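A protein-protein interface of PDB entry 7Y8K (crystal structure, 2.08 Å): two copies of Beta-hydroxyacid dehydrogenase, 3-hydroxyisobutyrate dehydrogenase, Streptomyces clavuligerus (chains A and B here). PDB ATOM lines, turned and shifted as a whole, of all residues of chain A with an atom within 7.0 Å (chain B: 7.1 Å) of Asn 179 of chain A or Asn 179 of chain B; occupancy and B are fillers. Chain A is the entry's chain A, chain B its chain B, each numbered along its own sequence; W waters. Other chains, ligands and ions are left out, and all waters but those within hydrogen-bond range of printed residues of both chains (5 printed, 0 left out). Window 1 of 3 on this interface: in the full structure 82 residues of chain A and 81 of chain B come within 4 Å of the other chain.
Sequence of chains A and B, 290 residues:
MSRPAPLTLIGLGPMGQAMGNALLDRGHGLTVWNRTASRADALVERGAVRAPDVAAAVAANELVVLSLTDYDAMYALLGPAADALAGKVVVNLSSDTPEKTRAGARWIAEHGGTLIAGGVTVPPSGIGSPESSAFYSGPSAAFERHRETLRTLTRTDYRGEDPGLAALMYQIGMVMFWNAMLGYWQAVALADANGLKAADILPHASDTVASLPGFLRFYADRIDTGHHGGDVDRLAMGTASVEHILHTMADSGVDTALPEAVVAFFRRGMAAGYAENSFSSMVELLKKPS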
ATOM      1  N   MET A 174      12.109 -20.551   1.910  1.00  0.00           N
ATOM      2  CA  MET A 174      12.473 -19.174   1.630  1.00  0.00           C
ATOM      3  C   MET A 174      11.519 -18.219   2.315  1.00  0.00           C
ATOM      4  O   MET A 174      11.939 -17.180   2.832  1.00  0.00           O
ATOM      5  CB  MET A 174      12.486 -18.931   0.114  1.00  0.00           C
ATOM      6  CG  MET A 174      13.801 -19.235  -0.623  1.00  0.00           C
ATOM      7  SD  MET A 174      15.318 -19.074   0.358  1.00  0.00           S
ATOM      8  CE  MET A 174      15.444 -17.307   0.363  1.00  0.00           C
ATOM      9  N   VAL A 175      10.228 -18.553   2.344  1.00  0.00           N
ATOM     10  CA  VAL A 175       9.296 -17.623   2.975  1.00  0.00           C
ATOM     11  C   VAL A 175       9.530 -17.543   4.485  1.00  0.00           C
ATOM     12  O   VAL A 175       9.293 -16.502   5.105  1.00  0.00           O
ATOM     13  CB  VAL A 175       7.848 -18.001   2.622  1.00  0.00           C
ATOM     14  CG1 VAL A 175       7.403 -19.212   3.408  1.00  0.00           C
ATOM     15  CG2 VAL A 175       6.939 -16.814   2.881  1.00  0.00           C
ATOM     16  N   MET A 176      10.029 -18.609   5.104  1.00  0.00           N
ATOM     17  CA  MET A 176      10.471 -18.489   6.487  1.00  0.00           C
ATOM     18  C   MET A 176      11.721 -17.603   6.579  1.00  0.00           C
ATOM     19  O   MET A 176      11.834 -16.736   7.456  1.00  0.00           O
ATOM     20  CB  MET A 176      10.716 -19.893   7.036  1.00  0.00           C
ATOM     21  CG  MET A 176       9.394 -20.661   7.263  1.00  0.00           C
ATOM     22  SD  MET A 176       9.590 -22.335   7.903  1.00  0.00           S
ATOM     23  CE  MET A 176      10.367 -21.979   9.480  1.00  0.00           C
ATOM     24  N   PHE A 177      12.665 -17.790   5.665  1.00  0.00           N
ATOM     25  CA  PHE A 177      13.901 -17.015   5.738  1.00  0.00           C
ATOM     26  C   PHE A 177      13.613 -15.535   5.623  1.00  0.00           C
ATOM     27  O   PHE A 177      13.969 -14.744   6.509  1.00  0.00           O
ATOM     28  CB  PHE A 177      14.872 -17.434   4.636  1.00  0.00           C
ATOM     29  CG  PHE A 177      16.145 -16.615   4.617  1.00  0.00           C
ATOM     30  CD1 PHE A 177      17.181 -16.908   5.492  1.00  0.00           C
ATOM     31  CD2 PHE A 177      16.284 -15.539   3.740  1.00  0.00           C
ATOM     32  CE1 PHE A 177      18.367 -16.153   5.492  1.00  0.00           C
ATOM     33  CE2 PHE A 177      17.447 -14.768   3.721  1.00  0.00           C
ATOM     34  CZ  PHE A 177      18.494 -15.076   4.595  1.00  0.00           C
ATOM     35  N   TRP A 178      12.975 -15.142   4.512  1.00  0.00           N
ATOM     36  CA  TRP A 178      12.757 -13.725   4.236  1.00  0.00           C
ATOM     37  C   TRP A 178      12.003 -13.058   5.370  1.00  0.00           C
ATOM     38  O   TRP A 178      12.374 -11.968   5.824  1.00  0.00           O
ATOM     39  CB  TRP A 178      11.999 -13.554   2.922  1.00  0.00           C
ATOM     40  CG  TRP A 178      12.753 -13.953   1.721  1.00  0.00           C
ATOM     41  CD1 TRP A 178      12.380 -14.888   0.786  1.00  0.00           C
ATOM     42  CD2 TRP A 178      14.018 -13.427   1.277  1.00  0.00           C
ATOM     43  NE1 TRP A 178      13.328 -14.967  -0.213  1.00  0.00           N
ATOM     44  CE2 TRP A 178      14.344 -14.082   0.067  1.00  0.00           C
ATOM     45  CE3 TRP A 178      14.899 -12.456   1.776  1.00  0.00           C
ATOM     46  CZ2 TRP A 178      15.515 -13.802  -0.638  1.00  0.00           C
ATOM     47  CZ3 TRP A 178      16.059 -12.187   1.072  1.00  0.00           C
ATOM     48  CH2 TRP A 178      16.355 -12.863  -0.117  1.00  0.00           C
ATOM     49  N   ASN A 179      10.955 -13.710   5.860  1.00  0.00           N
ATOM     50  CA  ASN A 179      10.104 -13.098   6.915  1.00  0.00           C
ATOM     51  C   ASN A 179      10.922 -12.894   8.194  1.00  0.00           C
ATOM     52  O   ASN A 179      10.841 -11.817   8.755  1.00  0.00           O
ATOM     53  CB  ASN A 179       8.801 -13.874   7.092  1.00  0.00           C
ATOM     54  CG  ASN A 179       7.759 -13.485   6.069  1.00  0.00           C
ATOM     55  OD1 ASN A 179       7.019 -12.530   6.260  1.00  0.00           O
ATOM     56  ND2 ASN A 179       7.718 -14.204   4.965  1.00  0.00           N
ATOM     57  N   ALA A 180      11.678 -13.892   8.609  1.00  0.00           N
ATOM     58  CA  ALA A 180      12.544 -13.771   9.801  1.00  0.00           C
ATOM     59  C   ALA A 180      13.551 -12.626   9.626  1.00  0.00           C
ATOM     60  O   ALA A 180      13.717 -11.853  10.543  1.00  0.00           O
ATOM     61  CB  ALA A 180      13.235 -15.080  10.035  1.00  0.00           C
ATOM     62  N   MET A 181      14.185 -12.558   8.465  1.00  0.00           N
ATOM     63  CA  MET A 181      15.199 -11.514   8.186  1.00  0.00           C
ATOM     64  C   MET A 181      14.551 -10.131   8.129  1.00  0.00           C
ATOM     65  O   MET A 181      15.203  -9.177   8.511  1.00  0.00           O
ATOM     66  CB  MET A 181      15.907 -11.826   6.873  1.00  0.00           C
ATOM     67  CG  MET A 181      16.853 -13.008   6.983  1.00  0.00           C
ATOM     68  SD  MET A 181      17.888 -13.028   8.465  1.00  0.00           S
ATOM     69  CE  MET A 181      19.195 -11.909   7.979  1.00  0.00           C
ATOM     70  N   LEU A 182      13.318 -10.064   7.660  1.00  0.00           N
ATOM     71  CA  LEU A 182      12.592  -8.776   7.602  1.00  0.00           C
ATOM     72  C   LEU A 182      12.283  -8.339   9.038  1.00  0.00           C
ATOM     73  O   LEU A 182      12.417  -7.163   9.310  1.00  0.00           O
ATOM     74  CB  LEU A 182      11.358  -8.896   6.704  1.00  0.00           C
ATOM     75  CG  LEU A 182      11.614  -8.824   5.200  1.00  0.00           C
ATOM     76  CD1 LEU A 182      10.316  -8.599   4.450  1.00  0.00           C
ATOM     77  CD2 LEU A 182      12.626  -7.751   4.854  1.00  0.00           C
ATOM     78  N   GLY A 183      11.914  -9.273   9.910  1.00  0.00           N
ATOM     79  CA  GLY A 183      11.738  -8.917  11.330  1.00  0.00           C
ATOM     80  C   GLY A 183      13.028  -8.343  11.893  1.00  0.00           C
ATOM     81  O   GLY A 183      12.948  -7.339  12.573  1.00  0.00           O
ATOM     82  N   TYR A 184      14.166  -8.955  11.579  1.00  0.00           N
ATOM     83  CA  TYR A 184      15.502  -8.489  12.033  1.00  0.00           C
ATOM     84  C   TYR A 184      15.819  -7.097  11.464  1.00  0.00           C
ATOM     85  O   TYR A 184      16.277  -6.274  12.215  1.00  0.00           O
ATOM     86  CB  TYR A 184      16.559  -9.517  11.632  1.00  0.00           C
ATOM     87  CG  TYR A 184      17.974  -9.256  12.079  1.00  0.00           C
ATOM     88  CD1 TYR A 184      18.268  -8.837  13.367  1.00  0.00           C
ATOM     89  CD2 TYR A 184      19.031  -9.469  11.212  1.00  0.00           C
ATOM     90  CE1 TYR A 184      19.573  -8.617  13.772  1.00  0.00           C
ATOM     91  CE2 TYR A 184      20.341  -9.254  11.599  1.00  0.00           C
ATOM     92  CZ  TYR A 184      20.612  -8.831  12.886  1.00  0.00           C
ATOM     93  OH  TYR A 184      21.901  -8.625  13.266  1.00  0.00           O
ATOM     94  N   TRP A 185      15.565  -6.885  10.172  1.00  0.00           N
ATOM     95  CA  TRP A 185      15.767  -5.557   9.534  1.00  0.00           C
ATOM     96  C   TRP A 185      14.980  -4.500  10.323  1.00  0.00           C
ATOM     97  O   TRP A 185      15.538  -3.458  10.610  1.00  0.00           O
ATOM     98  CB  TRP A 185      15.329  -5.606   8.068  1.00  0.00           C
ATOM     99  CG  TRP A 185      16.251  -6.184   7.035  1.00  0.00           C
ATOM    100  CD1 TRP A 185      16.057  -6.082   5.690  1.00  0.00           C
ATOM    101  CD2 TRP A 185      17.473  -6.933   7.202  1.00  0.00           C
ATOM    102  NE1 TRP A 185      17.060  -6.706   5.010  1.00  0.00           N
ATOM    103  CE2 TRP A 185      17.943  -7.233   5.907  1.00  0.00           C
ATOM    104  CE3 TRP A 185      18.231  -7.372   8.294  1.00  0.00           C
ATOM    105  CZ2 TRP A 185      19.112  -7.952   5.686  1.00  0.00           C
ATOM    106  CZ3 TRP A 185      19.386  -8.082   8.074  1.00  0.00           C
ATOM    107  CH2 TRP A 185      19.819  -8.371   6.785  1.00  0.00           C
ATOM    108  N   GLN A 186      13.736  -4.823  10.681  1.00  0.00           N
ATOM    109  CA  GLN A 186      12.865  -3.873  11.406  1.00  0.00           C
ATOM    110  C   GLN A 186      13.475  -3.587  12.776  1.00  0.00           C
ATOM    111  O   GLN A 186      13.508  -2.436  13.163  1.00  0.00           O
ATOM    112  CB  GLN A 186      11.445  -4.435  11.434  1.00  0.00           C
ATOM    113  CG  GLN A 186      10.772  -4.460  10.070  1.00  0.00           C
ATOM    114  CD  GLN A 186       9.420  -5.127  10.119  1.00  0.00           C
ATOM    115  OE1 GLN A 186       8.438  -4.540  10.552  1.00  0.00           O
ATOM    116  NE2 GLN A 186       9.363  -6.372   9.681  1.00  0.00           N
ATOM    117  N   ILE A 245       4.090  -2.779  18.339  1.00  0.00           N
ATOM    118  CA  ILE A 245       5.291  -2.730  17.507  1.00  0.00           C
ATOM    119  C   ILE A 245       5.124  -1.695  16.398  1.00  0.00           C
ATOM    120  O   ILE A 245       6.029  -0.899  16.114  1.00  0.00           O
ATOM    121  CB  ILE A 245       5.603  -4.121  16.923  1.00  0.00           C
ATOM    122  CG1 ILE A 245       6.037  -5.094  18.030  1.00  0.00           C
ATOM    123  CG2 ILE A 245       6.648  -3.999  15.788  1.00  0.00           C
ATOM    124  CD1 ILE A 245       5.637  -6.548  17.756  1.00  0.00           C
ATOM    125  N   LEU A 258       5.639  -2.501   6.651  1.00  0.00           N
ATOM    126  CA  LEU A 258       5.685  -3.908   7.054  1.00  0.00           C
ATOM    127  C   LEU A 258       4.888  -4.172   8.327  1.00  0.00           C
ATOM    128  O   LEU A 258       4.118  -5.153   8.361  1.00  0.00           O
ATOM    129  CB  LEU A 258       7.144  -4.362   7.193  1.00  0.00           C
ATOM    130  CG  LEU A 258       8.092  -4.341   5.987  1.00  0.00           C
ATOM    131  CD1 LEU A 258       9.468  -4.905   6.378  1.00  0.00           C
ATOM    132  CD2 LEU A 258       7.527  -5.081   4.769  1.00  0.00           C
ATOM    133  N   PRO A 259       5.022  -3.385   9.403  1.00  0.00           N
ATOM    134  CA  PRO A 259       4.171  -3.641  10.573  1.00  0.00           C
ATOM    135  C   PRO A 259       2.704  -3.385  10.308  1.00  0.00           C
ATOM    136  O   PRO A 259       1.868  -4.038  10.944  1.00  0.00           O
ATOM    137  CB  PRO A 259       4.728  -2.687  11.644  1.00  0.00           C
ATOM    138  CG  PRO A 259       5.504  -1.674  10.886  1.00  0.00           C
ATOM    139  CD  PRO A 259       6.076  -2.402   9.722  1.00  0.00           C
ATOM    140  N   VAL A 262       1.298  -6.479   9.012  1.00  0.00           N
ATOM    141  CA  VAL A 262       1.207  -7.449  10.104  1.00  0.00           C
ATOM    142  C   VAL A 262      -0.031  -7.178  10.957  1.00  0.00           C
ATOM    143  O   VAL A 262      -0.838  -8.081  11.215  1.00  0.00           O
ATOM    144  CB  VAL A 262       2.493  -7.432  10.946  1.00  0.00           C
ATOM    145  CG1 VAL A 262       2.272  -8.170  12.231  1.00  0.00           C
ATOM    146  CG2 VAL A 262       3.652  -8.058  10.140  1.00  0.00           C
ATOM    147  N   MET B 174      10.150  -8.782  19.941  1.00  0.00           N
ATOM    148  CA  MET B 174       8.839  -9.238  19.491  1.00  0.00           C
ATOM    149  C   MET B 174       8.673  -9.099  17.977  1.00  0.00           C
ATOM    150  O   MET B 174       8.165 -10.021  17.331  1.00  0.00           O
ATOM    151  CB  MET B 174       7.734  -8.510  20.248  1.00  0.00           C
ATOM    152  CG  MET B 174       7.607  -8.974  21.700  1.00  0.00           C
ATOM    153  SD  MET B 174       7.319 -10.762  21.896  1.00  0.00           S
ATOM    154  CE  MET B 174       8.710 -11.161  22.953  1.00  0.00           C
ATOM    155  N   VAL B 175       9.097  -7.977  17.382  1.00  0.00           N
ATOM    156  CA  VAL B 175       8.976  -7.843  15.918  1.00  0.00           C
ATOM    157  C   VAL B 175       9.739  -8.959  15.186  1.00  0.00           C
ATOM    158  O   VAL B 175       9.344  -9.383  14.095  1.00  0.00           O
ATOM    159  CB  VAL B 175       9.423  -6.426  15.464  1.00  0.00           C
ATOM    160  CG1 VAL B 175      10.945  -6.247  15.606  1.00  0.00           C
ATOM    161  CG2 VAL B 175       8.980  -6.137  14.042  1.00  0.00           C
ATOM    162  N   MET B 176      10.793  -9.505  15.791  1.00  0.00           N
ATOM    163  CA  MET B 176      11.456 -10.655  15.189  1.00  0.00           C
ATOM    164  C   MET B 176      10.652 -11.934  15.362  1.00  0.00           C
ATOM    165  O   MET B 176      10.615 -12.774  14.455  1.00  0.00           O
ATOM    166  CB  MET B 176      12.853 -10.815  15.797  1.00  0.00           C
ATOM    167  CG  MET B 176      13.658  -9.522  15.699  1.00  0.00           C
ATOM    168  SD  MET B 176      15.415  -9.661  15.969  1.00  0.00           S
ATOM    169  CE  MET B 176      15.905 -11.188  15.152  1.00  0.00           C
ATOM    170  N   PHE B 177       9.997 -12.113  16.506  1.00  0.00           N
ATOM    171  CA  PHE B 177       9.240 -13.366  16.780  1.00  0.00           C
ATOM    172  C   PHE B 177       8.051 -13.485  15.813  1.00  0.00           C
ATOM    173  O   PHE B 177       7.963 -14.474  15.101  1.00  0.00           O
ATOM    174  CB  PHE B 177       8.789 -13.430  18.240  1.00  0.00           C
ATOM    175  CG  PHE B 177       7.897 -14.598  18.576  1.00  0.00           C
ATOM    176  CD1 PHE B 177       8.430 -15.856  18.789  1.00  0.00           C
ATOM    177  CD2 PHE B 177       6.524 -14.443  18.671  1.00  0.00           C
ATOM    178  CE1 PHE B 177       7.611 -16.930  19.093  1.00  0.00           C
ATOM    179  CE2 PHE B 177       5.706 -15.519  18.974  1.00  0.00           C
ATOM    180  CZ  PHE B 177       6.251 -16.760  19.188  1.00  0.00           C
ATOM    181  N   TRP B 178       7.187 -12.476  15.803  1.00  0.00           N
ATOM    182  CA  TRP B 178       5.955 -12.468  14.972  1.00  0.00           C
ATOM    183  C   TRP B 178       6.274 -12.689  13.496  1.00  0.00           C
ATOM    184  O   TRP B 178       5.600 -13.489  12.910  1.00  0.00           O
ATOM    185  CB  TRP B 178       5.167 -11.190  15.222  1.00  0.00           C
ATOM    186  CG  TRP B 178       4.656 -10.995  16.612  1.00  0.00           C
ATOM    187  CD1 TRP B 178       4.894  -9.920  17.410  1.00  0.00           C
ATOM    188  CD2 TRP B 178       3.795 -11.865  17.365  1.00  0.00           C
ATOM    189  NE1 TRP B 178       4.253 -10.061  18.605  1.00  0.00           N
ATOM    190  CE2 TRP B 178       3.568 -11.241  18.608  1.00  0.00           C
ATOM    191  CE3 TRP B 178       3.196 -13.104  17.121  1.00  0.00           C
ATOM    192  CZ2 TRP B 178       2.780 -11.818  19.599  1.00  0.00           C
ATOM    193  CZ3 TRP B 178       2.417 -13.673  18.102  1.00  0.00           C
ATOM    194  CH2 TRP B 178       2.214 -13.039  19.325  1.00  0.00           C
ATOM    195  N   ASN B 179       7.292 -12.003  12.965  1.00  0.00           N
ATOM    196  CA  ASN B 179       7.662 -12.122  11.533  1.00  0.00           C
ATOM    197  C   ASN B 179       8.121 -13.548  11.217  1.00  0.00           C
ATOM    198  O   ASN B 179       7.615 -14.097  10.264  1.00  0.00           O
ATOM    199  CB  ASN B 179       8.662 -11.047  11.129  1.00  0.00           C
ATOM    200  CG  ASN B 179       7.951  -9.747  10.838  1.00  0.00           C
ATOM    201  OD1 ASN B 179       7.426  -9.578   9.753  1.00  0.00           O
ATOM    202  ND2 ASN B 179       7.872  -8.863  11.814  1.00  0.00           N
ATOM    203  N   ALA B 180       9.011 -14.108  12.018  1.00  0.00           N
ATOM    204  CA  ALA B 180       9.438 -15.516  11.843  1.00  0.00           C
ATOM    205  C   ALA B 180       8.244 -16.483  11.926  1.00  0.00           C
ATOM    206  O   ALA B 180       8.181 -17.388  11.120  1.00  0.00           O
ATOM    207  CB  ALA B 180      10.513 -15.841  12.840  1.00  0.00           C
ATOM    208  N   MET B 181       7.324 -16.252  12.859  1.00  0.00           N
ATOM    209  CA  MET B 181       6.191 -17.194  13.043  1.00  0.00           C
ATOM    210  C   MET B 181       5.174 -16.984  11.918  1.00  0.00           C
ATOM    211  O   MET B 181       4.561 -17.954  11.510  1.00  0.00           O
ATOM    212  CB  MET B 181       5.565 -17.030  14.425  1.00  0.00           C
ATOM    213  CG  MET B 181       6.490 -17.432  15.557  1.00  0.00           C
ATOM    214  SD  MET B 181       7.089 -19.138  15.495  1.00  0.00           S
ATOM    215  CE  MET B 181       5.576 -20.034  15.815  1.00  0.00           C
ATOM    216  N   LEU B 182       5.031 -15.761  11.435  1.00  0.00           N
ATOM    217  CA  LEU B 182       4.159 -15.505  10.265  1.00  0.00           C
ATOM    218  C   LEU B 182       4.774 -16.188   9.033  1.00  0.00           C
ATOM    219  O   LEU B 182       4.011 -16.737   8.252  1.00  0.00           O
ATOM    220  CB  LEU B 182       3.949 -13.998  10.109  1.00  0.00           C
ATOM    221  CG  LEU B 182       2.925 -13.381  11.058  1.00  0.00           C
ATOM    222  CD1 LEU B 182       2.439 -12.047  10.536  1.00  0.00           C
ATOM    223  CD2 LEU B 182       1.756 -14.316  11.298  1.00  0.00           C
ATOM    224  N   GLY B 183       6.101 -16.183   8.894  1.00  0.00           N
ATOM    225  CA  GLY B 183       6.765 -16.942   7.813  1.00  0.00           C
ATOM    226  C   GLY B 183       6.469 -18.427   7.932  1.00  0.00           C
ATOM    227  O   GLY B 183       6.191 -19.036   6.914  1.00  0.00           O
ATOM    228  N   TYR B 184       6.451 -18.959   9.143  1.00  0.00           N
ATOM    229  CA  TYR B 184       6.104 -20.380   9.391  1.00  0.00           C
ATOM    230  C   TYR B 184       4.632 -20.652   9.052  1.00  0.00           C
ATOM    231  O   TYR B 184       4.375 -21.629   8.399  1.00  0.00           O
ATOM    232  CB  TYR B 184       6.423 -20.738  10.844  1.00  0.00           C
ATOM    233  CG  TYR B 184       6.230 -22.175  11.250  1.00  0.00           C
ATOM    234  CD1 TYR B 184       6.716 -23.219  10.482  1.00  0.00           C
ATOM    235  CD2 TYR B 184       5.601 -22.491  12.438  1.00  0.00           C
ATOM    236  CE1 TYR B 184       6.555 -24.536  10.873  1.00  0.00           C
ATOM    237  CE2 TYR B 184       5.423 -23.799  12.845  1.00  0.00           C
ATOM    238  CZ  TYR B 184       5.907 -24.825  12.060  1.00  0.00           C
ATOM    239  OH  TYR B 184       5.738 -26.113  12.458  1.00  0.00           O
ATOM    240  N   TRP B 185       3.726 -19.799   9.520  1.00  0.00           N
ATOM    241  CA  TRP B 185       2.273 -19.910   9.212  1.00  0.00           C
ATOM    242  C   TRP B 185       2.075 -20.028   7.692  1.00  0.00           C
ATOM    243  O   TRP B 185       1.349 -20.907   7.275  1.00  0.00           O
ATOM    244  CB  TRP B 185       1.540 -18.698   9.790  1.00  0.00           C
ATOM    245  CG  TRP B 185       1.233 -18.659  11.254  1.00  0.00           C
ATOM    246  CD1 TRP B 185       0.452 -17.716  11.850  1.00  0.00           C
ATOM    247  CD2 TRP B 185       1.678 -19.533  12.313  1.00  0.00           C
ATOM    248  NE1 TRP B 185       0.371 -17.939  13.192  1.00  0.00           N
ATOM    249  CE2 TRP B 185       1.108 -19.044  13.505  1.00  0.00           C
ATOM    250  CE3 TRP B 185       2.475 -20.679  12.394  1.00  0.00           C
ATOM    251  CZ2 TRP B 185       1.329 -19.646  14.740  1.00  0.00           C
ATOM    252  CZ3 TRP B 185       2.688 -21.274  13.614  1.00  0.00           C
ATOM    253  CH2 TRP B 185       2.118 -20.765  14.772  1.00  0.00           C
ATOM    254  N   GLN B 186       2.770 -19.190   6.921  1.00  0.00           N
ATOM    255  CA  GLN B 186       2.681 -19.197   5.440  1.00  0.00           C
ATOM    256  C   GLN B 186       3.195 -20.524   4.881  1.00  0.00           C
ATOM    257  O   GLN B 186       2.572 -21.049   3.980  1.00  0.00           O
ATOM    258  CB  GLN B 186       3.438 -17.982   4.920  1.00  0.00           C
ATOM    259  CG  GLN B 186       2.731 -16.674   5.231  1.00  0.00           C
ATOM    260  CD  GLN B 186       3.510 -15.487   4.728  1.00  0.00           C
ATOM    261  OE1 GLN B 186       3.543 -15.218   3.536  1.00  0.00           O
ATOM    262  NE2 GLN B 186       4.152 -14.777   5.638  1.00  0.00           N
ATOM    263  N   ILE B 245       7.604 -16.676  -4.243  1.00  0.00           N
ATOM    264  CA  ILE B 245       6.813 -17.092  -3.075  1.00  0.00           C
ATOM    265  C   ILE B 245       5.367 -16.634  -3.231  1.00  0.00           C
ATOM    266  O   ILE B 245       4.424 -17.426  -3.118  1.00  0.00           O
ATOM    267  CB  ILE B 245       7.423 -16.543  -1.770  1.00  0.00           C
ATOM    268  CG1 ILE B 245       8.691 -17.314  -1.383  1.00  0.00           C
ATOM    269  CG2 ILE B 245       6.380 -16.579  -0.627  1.00  0.00           C
ATOM    270  CD1 ILE B 245       9.789 -16.405  -0.748  1.00  0.00           C
ATOM    271  N   LEU B 258       0.065 -11.259   2.990  1.00  0.00           N
ATOM    272  CA  LEU B 258       1.388 -11.178   3.616  1.00  0.00           C
ATOM    273  C   LEU B 258       2.501 -11.187   2.576  1.00  0.00           C
ATOM    274  O   LEU B 258       3.392 -10.323   2.651  1.00  0.00           O
ATOM    275  CB  LEU B 258       1.558 -12.294   4.651  1.00  0.00           C
ATOM    276  CG  LEU B 258       0.715 -12.220   5.926  1.00  0.00           C
ATOM    277  CD1 LEU B 258       0.957 -13.445   6.820  1.00  0.00           C
ATOM    278  CD2 LEU B 258       0.933 -10.903   6.680  1.00  0.00           C
ATOM    279  N   PRO B 259       2.527 -12.102   1.598  1.00  0.00           N
ATOM    280  CA  PRO B 259       3.594 -12.039   0.590  1.00  0.00           C
ATOM    281  C   PRO B 259       3.469 -10.847  -0.322  1.00  0.00           C
ATOM    282  O   PRO B 259       4.469 -10.459  -0.927  1.00  0.00           O
ATOM    283  CB  PRO B 259       3.441 -13.358  -0.183  1.00  0.00           C
ATOM    284  CG  PRO B 259       2.033 -13.803   0.084  1.00  0.00           C
ATOM    285  CD  PRO B 259       1.723 -13.337   1.468  1.00  0.00           C
ATOM    286  N   VAL B 262       5.548  -8.136   1.442  1.00  0.00           N
ATOM    287  CA  VAL B 262       6.970  -8.420   1.270  1.00  0.00           C
ATOM    288  C   VAL B 262       7.415  -8.035  -0.135  1.00  0.00           C
ATOM    289  O   VAL B 262       8.462  -7.403  -0.319  1.00  0.00           O
ATOM    290  CB  VAL B 262       7.262  -9.903   1.576  1.00  0.00           C
ATOM    291  CG1 VAL B 262       8.689 -10.238   1.242  1.00  0.00           C
ATOM    292  CG2 VAL B 262       6.926 -10.240   3.071  1.00  0.00           C
HETATM  293  O   HOH W   1       5.482 -13.505   3.104  1.00  0.00           O
HETATM  294  O   HOH W   2       6.332  -6.279  10.866  1.00  0.00           O
HETATM  295  O   HOH W   3      13.051 -12.846  13.130  1.00  0.00           O
HETATM  296  O   HOH W   4       6.793  -7.399   8.623  1.00  0.00           O
HETATM  297  O   HOH W   5      10.697 -17.904   9.681  1.00  0.00           O
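O of Val 175 of chain B is in hydrogen-bond range of ND2 of Asn 179 of chain B (2.8 Å).
The backbone carbonyl oxygen (O) of Val 175 of chain A is in hydrogen-bond range of the side-chain amide nitrogen (ND2) of Asn 179 of chain A (2.8 Å).
The side-chain amide nitrogen of Gln 186 of chain B is in hydrogen-bond range of the backbone carbonyl oxygen of Leu 182 of chain B (3.3 Å).
NE2 of Gln 186 of chain A sits at hydrogen-bond distance from O of Leu 182 of chain A, 3.2 Å away.
O of Gly 183 of chain B touches CG1 of Val 175 of chain A, at 3.7 Å.
CD1 of Ile 245 of chain B touches CD1 of Trp 178 of chain A, at 3.4 Å.
Asn 179 of chain B touches Asn 179 of chain A.
Asn 179 of chain A touches Val 262 of chain B.
CA of Gly 183 of chain A touches O of Val 175 of chain B, 3.7 Å away.
OE1 of Gln 186 of chain A touches CG2 of Val 175 of chain B, at 3.9 Å.
Gln 186 of chain A touches Asn 179 of chain B.
Ile 245 of chain A touches Met 174 of chain B (CD1 to CB, 3.8 Å).
Trp 178 of chain B touches Ile 245 of chain A.
Of chain B, only Asn 179 (3.3 Å), Gly 183 (3.8 Å), Gln 186 (3.7 Å) and Val 262 (3.9 Å) come within 4 Å of Asn 179 of chain A.
Of chain A, only Asn 179 (3.3 Å), Gly 183 (3.7 Å) and Gln 186 (3.6 Å) come within 4 Å of Asn 179 of chain B.
Of the printed residues of chain A, Ile 245 of chain B touches Met 174, Val 175 and Trp 178.
Of the printed residues of chain A, Gly 183 of chain B touches Val 175 (3.7 Å), Met 176 (3.6 Å) and Asn 179 (3.8 Å).
Of the printed residues of chain B, Tyr 184 of chain A touches Met 176 (3.8 Å).
Printed residues of chain B within 4 Å of Trp 178 of chain A: Ile 245.
Of the printed residues of chain B, Met 174 of chain A touches Ile 245.
Met 181 of chain B touches none of the printed residues of chain A.
Leu 182 of chain B touches none of the printed residues of chain A.
The nearest residue of chain B that does not touch Asn 179 of chain A is Ala 180 of chain B (4.4 Å).
The nearest printed residue of chain A that does not touch Val 175 of chain B is Tyr 184 of chain A (5.5 Å).
Of the 17 printed residues of chain A, 11 touch a printed residue of chain B.
Hydrophobic or aromatic side chains of chain A that line the printed part of chain B: Met 174, Val 175, Met 176, Trp 178, Ala 180, Leu 182, Tyr 184 and Ile 245.
Val 175 of chain A touches Gly 183 of chain B, and with the chains exchanged Gly 183 of chain A touches Val 175 of chain B.
Val 175 of chain A touches Gln 186 of chain B, and with the chains exchanged Gln 186 of chain A touches Val 175 of chain B.
Asn 179 of chain A touches its own counterpart, Asn 179 of chain B.
Positions printed for both chains: 174, 175, 176, 177, 178, 179, 180, 181, 182, 183, 184, 185, 186, 245, 258, 259 and 262.
Water W4 lies within hydrogen-bond range of OD1 of Asn 179 of chain B (2.5 Å) and NE2 of Gln 186 of chain A (3.0 Å).
Water W2 bridges the side-chain amide oxygen (OE1) of Gln 186 of chain A and the side-chain amide nitrogen (ND2) of Asn 179 of chain B.
Water W5 bridges the backbone carbonyl oxygen (O) of Met 176 of chain A (2.8 Å) and the backbone carbonyl oxygen (O) of Ala 180 of chain B (2.9 Å).
Water W3 lies within hydrogen-bond range of O of Met 176 of chain B (2.8 Å) and O of Ala 180 of chain A (2.8 Å).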
